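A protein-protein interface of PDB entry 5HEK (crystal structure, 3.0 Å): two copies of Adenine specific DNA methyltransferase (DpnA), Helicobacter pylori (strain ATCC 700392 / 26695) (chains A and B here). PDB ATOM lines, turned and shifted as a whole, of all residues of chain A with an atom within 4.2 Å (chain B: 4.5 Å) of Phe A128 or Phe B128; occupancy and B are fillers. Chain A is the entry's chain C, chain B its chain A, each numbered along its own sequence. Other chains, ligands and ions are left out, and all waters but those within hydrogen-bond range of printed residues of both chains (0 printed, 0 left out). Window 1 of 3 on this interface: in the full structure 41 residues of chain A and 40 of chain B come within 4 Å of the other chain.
Phe A128 touches just these residues of chain B: Phe B105 and Phe B128. Printed residues of chain A within 4 Å of Phe B128: Phe A105, Gln A107 and Phe A128. Printed residues of chain A within 4 Å of Phe B105: Phe A128 (3.2 Å). Printed residues of chain A within 4 Å of Gln B107: Gln A107 (3.1 Å) and Thr A126 (3.9 Å). Of the printed residues of chain A, Thr B126 touches Gln A107. The nearest residue of chain B that does not touch Phe A128 is Gln B107 (4.4 Å). The nearest printed residue of chain A that does not touch Phe B128 is Thr A126 (6.1 Å). The nearest printed residue of chain A that does not touch Tyr B85 is Phe A128 (6.5 Å).
Printed residues of chain B that touch a printed residue of chain A: Tyr B85, Phe B105, Gln B107, Thr B126 and Phe B128. Of the 9 printed residues of chain A, 4 touch a printed residue of chain B. Hydrophobic or aromatic side chains of chain A within 4 Å of the printed part of chain B: Phe A105 and Phe A128.
N of Cys B83 sits at hydrogen-bond distance from O of Phe B128. O of Phe A128 sits at hydrogen-bond distance from N of Cys A83 (3.0 Å).
Phe A105 touches Tyr B85 (CD1 to CD1, 3.6 Å). CZ of Phe A105 touches CE2 of Phe B128, at 3.2 Å. Thr B126 touches Gln A107. Phe B128 touches Gln A107 (CZ to OE1, 3.7 Å). Thr A126 touches Gln B107. CE2 of Phe A128 touches CZ of Phe B105, at 3.2 Å. Phe B128 touches Phe A128.
The side-chain amide oxygen (OE1) of Gln A107 sits close to the side-chain amide oxygen (OE1) of Gln B107 (3.1 Å).
Phe A105 touches Phe B128, and with the chains exchanged Phe A128 touches Phe B105. Gln B107 touches its own counterpart, Gln A107. Gln A107 touches Thr B126, and with the chains exchanged Thr A126 touches Gln B107. Phe B128 touches its own counterpart, Phe A128. 9 positions are printed for both chains. Of the 8 pairs that touch across the chains among the printed residues, 6 have their exchanged pair printed and touching as well.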
ATOM      1  N   PHE A  82     -13.969  18.476  18.308  1.00  0.00           N
ATOM      2  CA  PHE A  82     -12.635  17.956  18.575  1.00  0.00           C
ATOM      3  C   PHE A  82     -12.239  18.251  20.020  1.00  0.00           C
ATOM      4  O   PHE A  82     -12.532  19.329  20.541  1.00  0.00           O
ATOM      5  CB  PHE A  82     -11.613  18.547  17.598  1.00  0.00           C
ATOM      6  CG  PHE A  82     -11.742  18.034  16.187  1.00  0.00           C
ATOM      7  CD1 PHE A  82     -12.959  18.046  15.530  1.00  0.00           C
ATOM      8  CD2 PHE A  82     -10.630  17.545  15.520  1.00  0.00           C
ATOM      9  CE1 PHE A  82     -13.069  17.576  14.240  1.00  0.00           C
ATOM     10  CE2 PHE A  82     -10.725  17.075  14.230  1.00  0.00           C
ATOM     11  CZ  PHE A  82     -11.950  17.090  13.587  1.00  0.00           C
ATOM     12  N   CYS A  83     -11.619  17.279  20.682  1.00  0.00           N
ATOM     13  CA  CYS A  83     -11.221  17.472  22.071  1.00  0.00           C
ATOM     14  C   CYS A  83     -10.093  16.550  22.511  1.00  0.00           C
ATOM     15  O   CYS A  83      -9.636  15.678  21.764  1.00  0.00           O
ATOM     16  CB  CYS A  83     -12.429  17.279  22.989  1.00  0.00           C
ATOM     17  SG  CYS A  83     -13.351  15.746  22.689  1.00  0.00           S
ATOM     18  N   PHE A 105     -17.950   8.788  19.734  1.00  0.00           N
ATOM     19  CA  PHE A 105     -16.733   9.560  19.571  1.00  0.00           C
ATOM     20  C   PHE A 105     -16.008   9.044  18.338  1.00  0.00           C
ATOM     21  O   PHE A 105     -16.086   7.860  18.014  1.00  0.00           O
ATOM     22  CB  PHE A 105     -15.845   9.424  20.797  1.00  0.00           C
ATOM     23  CG  PHE A 105     -15.312   8.041  20.973  1.00  0.00           C
ATOM     24  CD1 PHE A 105     -16.087   7.069  21.588  1.00  0.00           C
ATOM     25  CD2 PHE A 105     -14.066   7.694  20.486  1.00  0.00           C
ATOM     26  CE1 PHE A 105     -15.622   5.783  21.736  1.00  0.00           C
ATOM     27  CE2 PHE A 105     -13.597   6.410  20.634  1.00  0.00           C
ATOM     28  CZ  PHE A 105     -14.380   5.451  21.256  1.00  0.00           C
ATOM     29  N   ILE A 106     -15.297   9.923  17.653  1.00  0.00           N
ATOM     30  CA  ILE A 106     -14.487   9.504  16.525  1.00  0.00           C
ATOM     31  C   ILE A 106     -13.061   9.914  16.788  1.00  0.00           C
ATOM     32  O   ILE A 106     -12.793  10.779  17.635  1.00  0.00           O
ATOM     33  CB  ILE A 106     -14.940  10.118  15.197  1.00  0.00           C
ATOM     34  CG1 ILE A 106     -14.773  11.637  15.226  1.00  0.00           C
ATOM     35  CG2 ILE A 106     -16.373   9.742  14.895  1.00  0.00           C
ATOM     36  CD1 ILE A 106     -15.153  12.288  13.914  1.00  0.00           C
ATOM     37  N   GLN A 107     -12.148   9.275  16.070  1.00  0.00           N
ATOM     38  CA  GLN A 107     -10.730   9.527  16.227  1.00  0.00           C
ATOM     39  C   GLN A 107     -10.054   9.394  14.862  1.00  0.00           C
ATOM     40  O   GLN A 107     -10.616   8.768  13.953  1.00  0.00           O
ATOM     41  CB  GLN A 107     -10.153   8.553  17.258  1.00  0.00           C
ATOM     42  CG  GLN A 107     -10.341   7.088  16.856  1.00  0.00           C
ATOM     43  CD  GLN A 107      -9.945   6.110  17.944  1.00  0.00           C
ATOM     44  OE1 GLN A 107      -9.752   6.494  19.094  1.00  0.00           O
ATOM     45  NE2 GLN A 107      -9.846   4.834  17.589  1.00  0.00           N
ATOM     46  N   THR A 126      -2.795   9.866  18.077  1.00  0.00           N
ATOM     47  CA  THR A 126      -4.254   9.785  18.047  1.00  0.00           C
ATOM     48  C   THR A 126      -4.901  11.076  18.514  1.00  0.00           C
ATOM     49  O   THR A 126      -4.564  11.601  19.578  1.00  0.00           O
ATOM     50  CB  THR A 126      -4.782   8.640  18.928  1.00  0.00           C
ATOM     51  OG1 THR A 126      -4.175   7.386  18.551  1.00  0.00           O
ATOM     52  CG2 THR A 126      -6.297   8.555  18.807  1.00  0.00           C
ATOM     53  N   GLU A 127      -5.857  11.560  17.724  1.00  0.00           N
ATOM     54  CA  GLU A 127      -6.632  12.756  18.043  1.00  0.00           C
ATOM     55  C   GLU A 127      -8.117  12.398  18.161  1.00  0.00           C
ATOM     56  O   GLU A 127      -8.571  11.440  17.526  1.00  0.00           O
ATOM     57  CB  GLU A 127      -6.411  13.825  16.962  1.00  0.00           C
ATOM     58  CG  GLU A 127      -6.657  15.254  17.412  1.00  0.00           C
ATOM     59  CD  GLU A 127      -5.550  15.774  18.303  1.00  0.00           C
ATOM     60  OE1 GLU A 127      -4.704  16.540  17.797  1.00  0.00           O
ATOM     61  OE2 GLU A 127      -5.514  15.404  19.500  1.00  0.00           O
ATOM     62  N   PHE A 128      -8.862  13.127  18.995  1.00  0.00           N
ATOM     63  CA  PHE A 128     -10.286  12.824  19.207  1.00  0.00           C
ATOM     64  C   PHE A 128     -11.278  13.905  18.801  1.00  0.00           C
ATOM     65  O   PHE A 128     -10.950  15.094  18.749  1.00  0.00           O
ATOM     66  CB  PHE A 128     -10.551  12.502  20.670  1.00  0.00           C
ATOM     67  CG  PHE A 128     -10.038  11.177  21.090  1.00  0.00           C
ATOM     68  CD1 PHE A 128     -10.698  10.018  20.706  1.00  0.00           C
ATOM     69  CD2 PHE A 128      -8.907  11.078  21.880  1.00  0.00           C
ATOM     70  CE1 PHE A 128     -10.233   8.780  21.096  1.00  0.00           C
ATOM     71  CE2 PHE A 128      -8.435   9.847  22.278  1.00  0.00           C
ATOM     72  CZ  PHE A 128      -9.096   8.692  21.886  1.00  0.00           C
ATOM     73  N   ALA A 129     -12.505  13.467  18.534  1.00  0.00           N
ATOM     74  CA  ALA A 129     -13.645  14.369  18.384  1.00  0.00           C
ATOM     75  C   ALA A 129     -14.893  13.698  18.950  1.00  0.00           C
ATOM     76  O   ALA A 129     -15.050  12.477  18.844  1.00  0.00           O
ATOM     77  CB  ALA A 129     -13.857  14.769  16.920  1.00  0.00           C
ATOM     78  N   PHE B  82      -8.389   0.336  32.723  1.00  0.00           N
ATOM     79  CA  PHE B  82      -9.325   0.264  31.608  1.00  0.00           C
ATOM     80  C   PHE B  82     -10.589   1.077  31.915  1.00  0.00           C
ATOM     81  O   PHE B  82     -11.097   1.036  33.042  1.00  0.00           O
ATOM     82  CB  PHE B  82      -9.687  -1.191  31.335  1.00  0.00           C
ATOM     83  CG  PHE B  82      -8.541  -2.015  30.840  1.00  0.00           C
ATOM     84  CD1 PHE B  82      -8.265  -2.112  29.486  1.00  0.00           C
ATOM     85  CD2 PHE B  82      -7.738  -2.705  31.739  1.00  0.00           C
ATOM     86  CE1 PHE B  82      -7.206  -2.887  29.039  1.00  0.00           C
ATOM     87  CE2 PHE B  82      -6.678  -3.478  31.303  1.00  0.00           C
ATOM     88  CZ  PHE B  82      -6.410  -3.573  29.956  1.00  0.00           C
ATOM     89  N   CYS B  83     -11.079   1.840  30.939  1.00  0.00           N
ATOM     90  CA  CYS B  83     -12.285   2.636  31.166  1.00  0.00           C
ATOM     91  C   CYS B  83     -13.021   3.095  29.893  1.00  0.00           C
ATOM     92  O   CYS B  83     -12.635   2.793  28.751  1.00  0.00           O
ATOM     93  CB  CYS B  83     -11.952   3.848  32.030  1.00  0.00           C
ATOM     94  SG  CYS B  83     -10.557   4.774  31.421  1.00  0.00           S
ATOM     95  N   TYR B  85     -14.833   6.270  27.592  1.00  0.00           N
ATOM     96  CA  TYR B  85     -14.565   7.654  27.223  1.00  0.00           C
ATOM     97  C   TYR B  85     -15.489   8.627  27.948  1.00  0.00           C
ATOM     98  O   TYR B  85     -15.245   9.840  27.947  1.00  0.00           O
ATOM     99  CB  TYR B  85     -14.691   7.840  25.708  1.00  0.00           C
ATOM    100  CG  TYR B  85     -16.106   7.878  25.178  1.00  0.00           C
ATOM    101  CD1 TYR B  85     -16.848   6.713  25.046  1.00  0.00           C
ATOM    102  CD2 TYR B  85     -16.683   9.075  24.777  1.00  0.00           C
ATOM    103  CE1 TYR B  85     -18.130   6.737  24.546  1.00  0.00           C
ATOM    104  CE2 TYR B  85     -17.973   9.115  24.271  1.00  0.00           C
ATOM    105  CZ  TYR B  85     -18.690   7.940  24.159  1.00  0.00           C
ATOM    106  OH  TYR B  85     -19.973   7.968  23.663  1.00  0.00           O
ATOM    107  N   PHE B 105      -2.848   7.539  27.262  1.00  0.00           N
ATOM    108  CA  PHE B 105      -3.927   6.566  27.195  1.00  0.00           C
ATOM    109  C   PHE B 105      -3.569   5.546  26.126  1.00  0.00           C
ATOM    110  O   PHE B 105      -2.902   5.874  25.161  1.00  0.00           O
ATOM    111  CB  PHE B 105      -5.263   7.243  26.873  1.00  0.00           C
ATOM    112  CG  PHE B 105      -5.326   7.830  25.485  1.00  0.00           C
ATOM    113  CD1 PHE B 105      -4.797   9.090  25.228  1.00  0.00           C
ATOM    114  CD2 PHE B 105      -5.907   7.127  24.438  1.00  0.00           C
ATOM    115  CE1 PHE B 105      -4.843   9.640  23.959  1.00  0.00           C
ATOM    116  CE2 PHE B 105      -5.956   7.672  23.164  1.00  0.00           C
ATOM    117  CZ  PHE B 105      -5.418   8.932  22.928  1.00  0.00           C
ATOM    118  N   ILE B 106      -3.996   4.306  26.305  1.00  0.00           N
ATOM    119  CA  ILE B 106      -3.786   3.282  25.294  1.00  0.00           C
ATOM    120  C   ILE B 106      -5.128   2.712  24.895  1.00  0.00           C
ATOM    121  O   ILE B 106      -6.104   2.832  25.641  1.00  0.00           O
ATOM    122  CB  ILE B 106      -2.874   2.140  25.787  1.00  0.00           C
ATOM    123  CG1 ILE B 106      -3.501   1.453  27.001  1.00  0.00           C
ATOM    124  CG2 ILE B 106      -1.501   2.666  26.152  1.00  0.00           C
ATOM    125  CD1 ILE B 106      -2.686   0.291  27.533  1.00  0.00           C
ATOM    126  N   GLN B 107      -5.169   2.081  23.727  1.00  0.00           N
ATOM    127  CA  GLN B 107      -6.410   1.549  23.196  1.00  0.00           C
ATOM    128  C   GLN B 107      -6.161   0.245  22.458  1.00  0.00           C
ATOM    129  O   GLN B 107      -5.027  -0.068  22.095  1.00  0.00           O
ATOM    130  CB  GLN B 107      -7.063   2.560  22.248  1.00  0.00           C
ATOM    131  CG  GLN B 107      -6.204   2.897  21.028  1.00  0.00           C
ATOM    132  CD  GLN B 107      -6.796   4.001  20.170  1.00  0.00           C
ATOM    133  OE1 GLN B 107      -7.689   4.726  20.604  1.00  0.00           O
ATOM    134  NE2 GLN B 107      -6.295   4.137  18.946  1.00  0.00           N
ATOM    135  N   THR B 126     -13.649  -0.185  19.514  1.00  0.00           N
ATOM    136  CA  THR B 126     -12.492   0.298  20.257  1.00  0.00           C
ATOM    137  C   THR B 126     -12.697   0.369  21.770  1.00  0.00           C
ATOM    138  O   THR B 126     -13.737   0.832  22.228  1.00  0.00           O
ATOM    139  CB  THR B 126     -12.090   1.694  19.761  1.00  0.00           C
ATOM    140  OG1 THR B 126     -11.894   1.657  18.339  1.00  0.00           O
ATOM    141  CG2 THR B 126     -10.814   2.168  20.467  1.00  0.00           C
ATOM    142  N   GLU B 127     -11.723  -0.120  22.540  1.00  0.00           N
ATOM    143  CA  GLU B 127     -11.738   0.020  24.001  1.00  0.00           C
ATOM    144  C   GLU B 127     -10.508   0.781  24.479  1.00  0.00           C
ATOM    145  O   GLU B 127      -9.445   0.704  23.853  1.00  0.00           O
ATOM    146  CB  GLU B 127     -11.822  -1.347  24.662  1.00  0.00           C
ATOM    147  CG  GLU B 127     -13.151  -2.035  24.404  1.00  0.00           C
ATOM    148  CD  GLU B 127     -14.248  -1.556  25.334  1.00  0.00           C
ATOM    149  OE1 GLU B 127     -14.316  -0.339  25.613  1.00  0.00           O
ATOM    150  OE2 GLU B 127     -15.059  -2.399  25.771  1.00  0.00           O
ATOM    151  N   PHE B 128     -10.644   1.502  25.591  1.00  0.00           N
ATOM    152  CA  PHE B 128      -9.567   2.370  26.071  1.00  0.00           C
ATOM    153  C   PHE B 128      -9.001   1.942  27.402  1.00  0.00           C
ATOM    154  O   PHE B 128      -9.664   1.261  28.186  1.00  0.00           O
ATOM    155  CB  PHE B 128     -10.051   3.805  26.216  1.00  0.00           C
ATOM    156  CG  PHE B 128     -10.333   4.474  24.922  1.00  0.00           C
ATOM    157  CD1 PHE B 128      -9.296   4.897  24.102  1.00  0.00           C
ATOM    158  CD2 PHE B 128     -11.644   4.698  24.527  1.00  0.00           C
ATOM    159  CE1 PHE B 128      -9.565   5.522  22.897  1.00  0.00           C
ATOM    160  CE2 PHE B 128     -11.922   5.322  23.333  1.00  0.00           C
ATOM    161  CZ  PHE B 128     -10.884   5.736  22.509  1.00  0.00           C
ATOM    162  N   ALA B 129      -7.774   2.371  27.666  1.00  0.00           N
ATOM    163  CA  ALA B 129      -7.175   2.210  28.987  1.00  0.00           C
ATOM    164  C   ALA B 129      -6.367   3.450  29.329  1.00  0.00           C
ATOM    165  O   ALA B 129      -5.817   4.107  28.439  1.00  0.00           O
ATOM    166  CB  ALA B 129      -6.288   0.949  29.047  1.00  0.00           C
